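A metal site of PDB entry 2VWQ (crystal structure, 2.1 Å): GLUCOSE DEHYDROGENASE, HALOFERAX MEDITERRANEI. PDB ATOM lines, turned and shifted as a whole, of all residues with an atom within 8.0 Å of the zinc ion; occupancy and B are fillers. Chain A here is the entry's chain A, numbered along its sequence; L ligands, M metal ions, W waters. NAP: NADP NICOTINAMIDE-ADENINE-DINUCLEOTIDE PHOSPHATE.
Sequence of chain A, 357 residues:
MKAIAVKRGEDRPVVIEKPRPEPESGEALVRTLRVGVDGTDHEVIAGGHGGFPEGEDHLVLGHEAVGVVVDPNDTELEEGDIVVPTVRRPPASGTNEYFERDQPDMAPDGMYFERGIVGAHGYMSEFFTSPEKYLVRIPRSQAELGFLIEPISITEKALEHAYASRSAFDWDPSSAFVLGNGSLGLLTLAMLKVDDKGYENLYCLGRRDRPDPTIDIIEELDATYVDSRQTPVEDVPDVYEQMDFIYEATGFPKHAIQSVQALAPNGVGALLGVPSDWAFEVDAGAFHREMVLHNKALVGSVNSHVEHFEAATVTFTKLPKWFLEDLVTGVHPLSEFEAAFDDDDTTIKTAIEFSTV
The backbone NH (N) of Leu 184 is in hydrogen-bond range of an oxygen (O1N) of the ligand (3.2 Å). The backbone NH of Ser 183 sits at hydrogen-bond distance from an oxygen (O1N) of the ligand (3.4 Å).
The side-chain carboxylate of Glu 64 is in salt-bridge range of the side-chain amino group of Lys 349 (2.6 Å). The backbone carbonyl oxygen (O) of Glu 64 is in hydrogen-bond range of the backbone NH (N) of Gly 36 (2.8 Å). O of Glu 150 sits at hydrogen-bond distance from OG of Ser 153 (2.6 Å). N of Thr 40 is in hydrogen-bond range of OD1 of Asp 38, 2.9 Å away. The side-chain carboxylate (OD2) of Asp 41 is in hydrogen-bond range of the backbone NH (N) of Asp 38 (3.1 Å).
Residues that only touch the zinc ion: Asp 38. Of the 23 residues printed, 4 come within 4 Å of the zinc ion. The nearest printed residue that does not touch the zinc ion is Pro 151 (4.6 Å).
Water W1 binds the zinc ion, 1.7 Å away. A ring nitrogen (NE2) of His 63 is bound to the zinc ion, 2.1 Å away. OE2 of Glu 64 binds the zinc ion (2.3 Å). OE1 of Glu 150 binds the zinc ion.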
ATOM      1  N   GLY A  36      -2.249  -3.636 -10.327  1.00  0.00           N
ATOM      2  CA  GLY A  36      -3.372  -3.270 -11.191  1.00  0.00           C
ATOM      3  C   GLY A  36      -3.034  -3.465 -12.652  1.00  0.00           C
ATOM      4  O   GLY A  36      -1.860  -3.532 -13.014  1.00  0.00           O
ATOM      5  N   VAL A  37      -4.054  -3.591 -13.496  1.00  0.00           N
ATOM      6  CA  VAL A  37      -3.876  -3.698 -14.950  1.00  0.00           C
ATOM      7  C   VAL A  37      -4.463  -2.425 -15.527  1.00  0.00           C
ATOM      8  O   VAL A  37      -5.563  -2.060 -15.161  1.00  0.00           O
ATOM      9  CB  VAL A  37      -4.679  -4.917 -15.508  1.00  0.00           C
ATOM     10  CG1 VAL A  37      -4.582  -5.001 -17.044  1.00  0.00           C
ATOM     11  CG2 VAL A  37      -4.225  -6.222 -14.868  1.00  0.00           C
ATOM     12  N   ASP A  38      -3.740  -1.702 -16.403  1.00  0.00           N
ATOM     13  CA  ASP A  38      -4.415  -0.683 -17.228  1.00  0.00           C
ATOM     14  C   ASP A  38      -4.167  -0.863 -18.743  1.00  0.00           C
ATOM     15  O   ASP A  38      -3.597  -1.885 -19.166  1.00  0.00           O
ATOM     16  CB  ASP A  38      -4.250   0.780 -16.702  1.00  0.00           C
ATOM     17  CG  ASP A  38      -2.973   1.473 -17.131  1.00  0.00           C
ATOM     18  OD1 ASP A  38      -2.201   0.965 -17.942  1.00  0.00           O
ATOM     19  OD2 ASP A  38      -2.705   2.567 -16.617  1.00  0.00           O
ATOM     20  N   GLY A  39      -4.672   0.099 -19.523  1.00  0.00           N
ATOM     21  CA  GLY A  39      -4.578   0.084 -20.983  1.00  0.00           C
ATOM     22  C   GLY A  39      -3.184  -0.189 -21.495  1.00  0.00           C
ATOM     23  O   GLY A  39      -2.993  -0.957 -22.431  1.00  0.00           O
ATOM     24  N   THR A  40      -2.202   0.411 -20.817  1.00  0.00           N
ATOM     25  CA  THR A  40      -0.816   0.261 -21.214  1.00  0.00           C
ATOM     26  C   THR A  40      -0.338  -1.177 -21.153  1.00  0.00           C
ATOM     27  O   THR A  40       0.441  -1.598 -21.996  1.00  0.00           O
ATOM     28  CB  THR A  40       0.068   1.188 -20.335  1.00  0.00           C
ATOM     29  OG1 THR A  40      -0.464   2.524 -20.355  1.00  0.00           O
ATOM     30  CG2 THR A  40       1.486   1.213 -20.826  1.00  0.00           C
ATOM     31  N   ASP A  41      -0.825  -1.946 -20.190  1.00  0.00           N
ATOM     32  CA  ASP A  41      -0.510  -3.375 -20.148  1.00  0.00           C
ATOM     33  C   ASP A  41      -1.104  -4.116 -21.348  1.00  0.00           C
ATOM     34  O   ASP A  41      -0.478  -5.023 -21.906  1.00  0.00           O
ATOM     35  CB  ASP A  41      -1.036  -4.003 -18.846  1.00  0.00           C
ATOM     36  CG  ASP A  41      -0.317  -3.482 -17.617  1.00  0.00           C
ATOM     37  OD1 ASP A  41       0.798  -3.994 -17.362  1.00  0.00           O
ATOM     38  OD2 ASP A  41      -0.848  -2.547 -16.955  1.00  0.00           O
ATOM     39  N   GLY A  62       3.040  -4.915 -15.675  1.00  0.00           N
ATOM     40  CA  GLY A  62       2.500  -4.267 -14.467  1.00  0.00           C
ATOM     41  C   GLY A  62       3.336  -3.101 -13.977  1.00  0.00           C
ATOM     42  O   GLY A  62       4.532  -3.246 -13.710  1.00  0.00           O
ATOM     43  N   HIS A  63       2.698  -1.940 -13.825  1.00  0.00           N
ATOM     44  CA  HIS A  63       3.362  -0.759 -13.298  1.00  0.00           C
ATOM     45  C   HIS A  63       2.649  -0.099 -12.107  1.00  0.00           C
ATOM     46  O   HIS A  63       3.159   0.877 -11.560  1.00  0.00           O
ATOM     47  CB  HIS A  63       3.591   0.277 -14.409  1.00  0.00           C
ATOM     48  CG  HIS A  63       2.337   0.908 -14.929  1.00  0.00           C
ATOM     49  ND1 HIS A  63       1.632   0.373 -15.979  1.00  0.00           N
ATOM     50  CD2 HIS A  63       1.689   2.038 -14.575  1.00  0.00           C
ATOM     51  CE1 HIS A  63       0.584   1.138 -16.235  1.00  0.00           C
ATOM     52  NE2 HIS A  63       0.596   2.168 -15.409  1.00  0.00           N
ATOM     53  N   GLU A  64       1.501  -0.637 -11.727  1.00  0.00           N
ATOM     54  CA  GLU A  64       0.692  -0.121 -10.644  1.00  0.00           C
ATOM     55  C   GLU A  64       0.726  -1.129  -9.514  1.00  0.00           C
ATOM     56  O   GLU A  64      -0.048  -2.078  -9.503  1.00  0.00           O
ATOM     57  CB  GLU A  64      -0.765   0.059 -11.118  1.00  0.00           C
ATOM     58  CG  GLU A  64      -0.920   0.908 -12.331  1.00  0.00           C
ATOM     59  CD  GLU A  64      -2.353   1.068 -12.806  1.00  0.00           C
ATOM     60  OE1 GLU A  64      -3.228   0.273 -12.399  1.00  0.00           O
ATOM     61  OE2 GLU A  64      -2.612   2.000 -13.607  1.00  0.00           O
ATOM     62  N   ALA A  65       1.626  -0.947  -8.553  1.00  0.00           N
ATOM     63  CA  ALA A  65       1.816  -1.978  -7.541  1.00  0.00           C
ATOM     64  C   ALA A  65       1.775  -1.451  -6.123  1.00  0.00           C
ATOM     65  O   ALA A  65       2.022  -0.272  -5.865  1.00  0.00           O
ATOM     66  CB  ALA A  65       3.131  -2.678  -7.789  1.00  0.00           C
ATOM     67  N   VAL A  87       7.465   4.547 -11.182  1.00  0.00           N
ATOM     68  CA  VAL A  87       7.590   3.763 -12.402  1.00  0.00           C
ATOM     69  C   VAL A  87       8.907   4.003 -13.148  1.00  0.00           C
ATOM     70  O   VAL A  87       9.488   3.065 -13.703  1.00  0.00           O
ATOM     71  CB  VAL A  87       6.362   4.019 -13.305  1.00  0.00           C
ATOM     72  CG1 VAL A  87       6.439   3.193 -14.651  1.00  0.00           C
ATOM     73  CG2 VAL A  87       5.093   3.690 -12.521  1.00  0.00           C
ATOM     74  N   ILE A 117       6.693  -1.196 -18.736  1.00  0.00           N
ATOM     75  CA  ILE A 117       6.237  -0.476 -19.943  1.00  0.00           C
ATOM     76  C   ILE A 117       7.367  -0.391 -20.985  1.00  0.00           C
ATOM     77  O   ILE A 117       7.231  -0.892 -22.091  1.00  0.00           O
ATOM     78  CB  ILE A 117       5.733   0.944 -19.603  1.00  0.00           C
ATOM     79  CG1 ILE A 117       4.624   0.897 -18.537  1.00  0.00           C
ATOM     80  CG2 ILE A 117       5.219   1.652 -20.876  1.00  0.00           C
ATOM     81  CD1 ILE A 117       4.131   2.297 -18.083  1.00  0.00           C
ATOM     82  N   PHE A 147      -2.788  -0.260  -5.321  1.00  0.00           N
ATOM     83  CA  PHE A 147      -2.426  -0.168  -6.736  1.00  0.00           C
ATOM     84  C   PHE A 147      -3.118   1.023  -7.417  1.00  0.00           C
ATOM     85  O   PHE A 147      -2.792   1.351  -8.562  1.00  0.00           O
ATOM     86  CB  PHE A 147      -2.772  -1.474  -7.471  1.00  0.00           C
ATOM     87  CG  PHE A 147      -4.224  -1.871  -7.346  1.00  0.00           C
ATOM     88  CD1 PHE A 147      -5.158  -1.397  -8.241  1.00  0.00           C
ATOM     89  CD2 PHE A 147      -4.637  -2.698  -6.330  1.00  0.00           C
ATOM     90  CE1 PHE A 147      -6.500  -1.731  -8.128  1.00  0.00           C
ATOM     91  CE2 PHE A 147      -5.976  -3.054  -6.210  1.00  0.00           C
ATOM     92  CZ  PHE A 147      -6.904  -2.561  -7.113  1.00  0.00           C
ATOM     93  N   LEU A 148      -4.085   1.640  -6.728  1.00  0.00           N
ATOM     94  CA  LEU A 148      -4.740   2.832  -7.256  1.00  0.00           C
ATOM     95  C   LEU A 148      -3.946   4.117  -7.038  1.00  0.00           C
ATOM     96  O   LEU A 148      -4.269   5.154  -7.624  1.00  0.00           O
ATOM     97  CB  LEU A 148      -6.150   3.000  -6.658  1.00  0.00           C
ATOM     98  CG  LEU A 148      -7.209   2.004  -7.128  1.00  0.00           C
ATOM     99  CD1 LEU A 148      -8.546   2.328  -6.464  1.00  0.00           C
ATOM    100  CD2 LEU A 148      -7.344   2.019  -8.660  1.00  0.00           C
ATOM    101  N   ILE A 149      -2.914   4.055  -6.197  1.00  0.00           N
ATOM    102  CA  ILE A 149      -2.143   5.261  -5.867  1.00  0.00           C
ATOM    103  C   ILE A 149      -1.424   5.774  -7.110  1.00  0.00           C
ATOM    104  O   ILE A 149      -1.365   6.984  -7.324  1.00  0.00           O
ATOM    105  CB  ILE A 149      -1.132   4.987  -4.725  1.00  0.00           C
ATOM    106  CG1 ILE A 149      -1.883   4.672  -3.420  1.00  0.00           C
ATOM    107  CG2 ILE A 149      -0.173   6.197  -4.509  1.00  0.00           C
ATOM    108  CD1 ILE A 149      -2.778   5.755  -2.940  1.00  0.00           C
ATOM    109  N   GLU A 150      -0.883   4.878  -7.933  1.00  0.00           N
ATOM    110  CA  GLU A 150      -0.207   5.319  -9.138  1.00  0.00           C
ATOM    111  C   GLU A 150      -1.140   6.073 -10.098  1.00  0.00           C
ATOM    112  O   GLU A 150      -0.825   7.190 -10.513  1.00  0.00           O
ATOM    113  CB  GLU A 150       0.569   4.168  -9.778  1.00  0.00           C
ATOM    114  CG  GLU A 150       1.529   4.561 -10.865  1.00  0.00           C
ATOM    115  CD  GLU A 150       0.886   4.708 -12.231  1.00  0.00           C
ATOM    116  OE1 GLU A 150      -0.230   4.222 -12.422  1.00  0.00           O
ATOM    117  OE2 GLU A 150       1.517   5.315 -13.126  1.00  0.00           O
ATOM    118  N   PRO A 151      -2.271   5.474 -10.498  1.00  0.00           N
ATOM    119  CA  PRO A 151      -3.162   6.279 -11.391  1.00  0.00           C
ATOM    120  C   PRO A 151      -3.681   7.609 -10.805  1.00  0.00           C
ATOM    121  O   PRO A 151      -3.787   8.619 -11.526  1.00  0.00           O
ATOM    122  CB  PRO A 151      -4.299   5.302 -11.722  1.00  0.00           C
ATOM    123  CG  PRO A 151      -4.208   4.203 -10.754  1.00  0.00           C
ATOM    124  CD  PRO A 151      -2.765   4.100 -10.347  1.00  0.00           C
ATOM    125  N   ILE A 152      -3.972   7.641  -9.522  1.00  0.00           N
ATOM    126  CA  ILE A 152      -4.360   8.880  -8.845  1.00  0.00           C
ATOM    127  C   ILE A 152      -3.249   9.918  -9.003  1.00  0.00           C
ATOM    128  O   ILE A 152      -3.532  11.098  -9.243  1.00  0.00           O
ATOM    129  CB  ILE A 152      -4.718   8.651  -7.350  1.00  0.00           C
ATOM    130  CG1 ILE A 152      -6.010   7.833  -7.236  1.00  0.00           C
ATOM    131  CG2 ILE A 152      -4.949   9.988  -6.624  1.00  0.00           C
ATOM    132  CD1 ILE A 152      -6.329   7.351  -5.819  1.00  0.00           C
ATOM    133  N   SER A 153      -1.989   9.471  -8.881  1.00  0.00           N
ATOM    134  CA  SER A 153      -0.826  10.364  -8.970  1.00  0.00           C
ATOM    135  C   SER A 153      -0.652  10.988 -10.349  1.00  0.00           C
ATOM    136  O   SER A 153      -0.166  12.107 -10.464  1.00  0.00           O
ATOM    137  CB  SER A 153       0.468   9.649  -8.533  1.00  0.00           C
ATOM    138  OG  SER A 153       0.960   8.758  -9.530  1.00  0.00           O
ATOM    139  N   ILE A 154      -1.036  10.241 -11.391  1.00  0.00           N
ATOM    140  CA  ILE A 154      -1.042  10.734 -12.757  1.00  0.00           C
ATOM    141  C   ILE A 154      -1.889  12.011 -12.824  1.00  0.00           C
ATOM    142  O   ILE A 154      -1.459  13.049 -13.335  1.00  0.00           O
ATOM    143  CB  ILE A 154      -1.567   9.664 -13.752  1.00  0.00           C
ATOM    144  CG1 ILE A 154      -0.584   8.454 -13.872  1.00  0.00           C
ATOM    145  CG2 ILE A 154      -1.799  10.255 -15.137  1.00  0.00           C
ATOM    146  CD1 ILE A 154       0.849   8.809 -14.330  1.00  0.00           C
ATOM    147  N   SER A 183     -10.837   3.856 -16.613  1.00  0.00           N
ATOM    148  CA  SER A 183     -10.506   3.889 -15.191  1.00  0.00           C
ATOM    149  C   SER A 183      -9.825   5.230 -14.804  1.00  0.00           C
ATOM    150  O   SER A 183     -10.124   5.755 -13.748  1.00  0.00           O
ATOM    151  CB  SER A 183      -9.635   2.695 -14.796  1.00  0.00           C
ATOM    152  OG  SER A 183      -8.429   2.704 -15.526  1.00  0.00           O
ATOM    153  N   LEU A 184      -8.982   5.783 -15.668  1.00  0.00           N
ATOM    154  CA  LEU A 184      -8.386   7.108 -15.425  1.00  0.00           C
ATOM    155  C   LEU A 184      -9.407   8.250 -15.435  1.00  0.00           C
ATOM    156  O   LEU A 184      -9.365   9.128 -14.598  1.00  0.00           O
ATOM    157  CB  LEU A 184      -7.268   7.428 -16.436  1.00  0.00           C
ATOM    158  CG  LEU A 184      -6.401   8.665 -16.124  1.00  0.00           C
ATOM    159  CD1 LEU A 184      -5.681   8.525 -14.763  1.00  0.00           C
ATOM    160  CD2 LEU A 184      -5.421   8.989 -17.249  1.00  0.00           C
ATOM    161  N   LYS A 349     -11.807  -1.564 -13.615  1.00  0.00           N
ATOM    162  CA  LYS A 349     -10.433  -1.706 -13.140  1.00  0.00           C
ATOM    163  C   LYS A 349     -10.280  -3.070 -12.539  1.00  0.00           C
ATOM    164  O   LYS A 349     -11.062  -3.464 -11.684  1.00  0.00           O
ATOM    165  CB  LYS A 349     -10.101  -0.652 -12.090  1.00  0.00           C
ATOM    166  CG  LYS A 349      -8.634  -0.655 -11.648  1.00  0.00           C
ATOM    167  CD  LYS A 349      -7.760  -0.211 -12.782  1.00  0.00           C
ATOM    168  CE  LYS A 349      -6.359   0.071 -12.364  1.00  0.00           C
ATOM    169  NZ  LYS A 349      -5.567   0.475 -13.569  1.00  0.00           N
HETATM  170  PA  NAP L   1      -9.111   3.192 -21.430  1.00  0.00           P
HETATM  171  O1A NAP L   1      -9.428   2.191 -20.404  1.00  0.00           O
HETATM  172  O2A NAP L   1      -8.914   2.764 -22.798  1.00  0.00           O
HETATM  173  O5B NAP L   1     -10.246   4.310 -21.418  1.00  0.00           O
HETATM  174  C5B NAP L   1     -10.462   5.066 -22.579  1.00  0.00           C
HETATM  175  C4B NAP L   1     -11.937   5.355 -22.645  1.00  0.00           C
HETATM  176  O4B NAP L   1     -12.137   6.368 -23.603  1.00  0.00           O
HETATM  177  C3B NAP L   1     -12.754   4.124 -23.063  1.00  0.00           C
HETATM  178  O3B NAP L   1     -13.719   3.845 -22.080  1.00  0.00           O
HETATM  179  C2B NAP L   1     -13.383   4.562 -24.381  1.00  0.00           C
HETATM  180  O2B NAP L   1     -14.712   4.126 -24.535  1.00  0.00           O
HETATM  181  C1B NAP L   1     -13.314   6.079 -24.286  1.00  0.00           C
HETATM  182  N9A NAP L   1     -13.305   6.676 -25.615  1.00  0.00           N
HETATM  183  C8A NAP L   1     -12.396   6.491 -26.627  1.00  0.00           C
HETATM  184  N7A NAP L   1     -12.805   7.213 -27.694  1.00  0.00           N
HETATM  185  C5A NAP L   1     -13.970   7.838 -27.355  1.00  0.00           C
HETATM  186  C6A NAP L   1     -14.796   8.686 -28.029  1.00  0.00           C
HETATM  187  N6A NAP L   1     -14.511   9.037 -29.279  1.00  0.00           N
HETATM  188  N1A NAP L   1     -15.921   9.183 -27.415  1.00  0.00           N
HETATM  189  C2A NAP L   1     -16.218   8.834 -26.117  1.00  0.00           C
HETATM  190  N3A NAP L   1     -15.387   7.973 -25.441  1.00  0.00           N
HETATM  191  C4A NAP L   1     -14.283   7.500 -26.046  1.00  0.00           C
HETATM  192  O3  NAP L   1      -7.790   3.903 -20.874  1.00  0.00           O
HETATM  193  PN  NAP L   1      -7.446   4.544 -19.439  1.00  0.00           P
HETATM  194  O1N NAP L   1      -8.622   5.204 -18.801  1.00  0.00           O
HETATM  195  O2N NAP L   1      -6.656   3.613 -18.593  1.00  0.00           O
HETATM  196  O5D NAP L   1      -6.472   5.652 -20.120  1.00  0.00           O
HETATM  197  C5D NAP L   1      -7.034   6.636 -20.968  1.00  0.00           C
HETATM  198  C4D NAP L   1      -5.993   7.248 -21.892  1.00  0.00           C
HETATM  199  O4D NAP L   1      -4.982   7.838 -21.088  1.00  0.00           O
HETATM  200  C3D NAP L   1      -5.264   6.261 -22.808  1.00  0.00           C
HETATM  201  O3D NAP L   1      -4.976   6.866 -24.049  1.00  0.00           O
HETATM  202  C2D NAP L   1      -3.967   5.988 -22.096  1.00  0.00           C
HETATM  203  O2D NAP L   1      -2.920   5.688 -22.988  1.00  0.00           O
HETATM  204  C1D NAP L   1      -3.709   7.336 -21.459  1.00  0.00           C
HETATM  205  N1N NAP L   1      -2.886   7.357 -20.251  1.00  0.00           N
HETATM  206  C2N NAP L   1      -1.901   8.308 -20.185  1.00  0.00           C
HETATM  207  C3N NAP L   1      -1.119   8.392 -19.042  1.00  0.00           C
HETATM  208  C7N NAP L   1      -0.167   9.555 -18.885  1.00  0.00           C
HETATM  209  O7N NAP L   1       0.795   9.469 -17.893  1.00  0.00           O
HETATM  210  N7N NAP L   1      -0.268  10.629 -19.664  1.00  0.00           N
HETATM  211  C4N NAP L   1      -1.363   7.534 -17.979  1.00  0.00           C
HETATM  212  C5N NAP L   1      -2.396   6.603 -18.060  1.00  0.00           C
HETATM  213  C6N NAP L   1      -3.155   6.529 -19.213  1.00  0.00           C
HETATM  214  P2B NAP L   1     -15.078   2.690 -25.218  1.00  0.00           P
HETATM  215  O1X NAP L   1     -14.588   1.653 -24.286  1.00  0.00           O
HETATM  216  O2X NAP L   1     -14.369   2.545 -26.535  1.00  0.00           O
HETATM  217  O3X NAP L   1     -16.576   2.697 -25.343  1.00  0.00           O
HETATM  218 ZN    ZN M   1      -0.953   3.330 -14.479  1.00  0.00          ZN
HETATM  219  O   HOH W   1      -1.077   4.177 -15.954  1.00  0.00           O
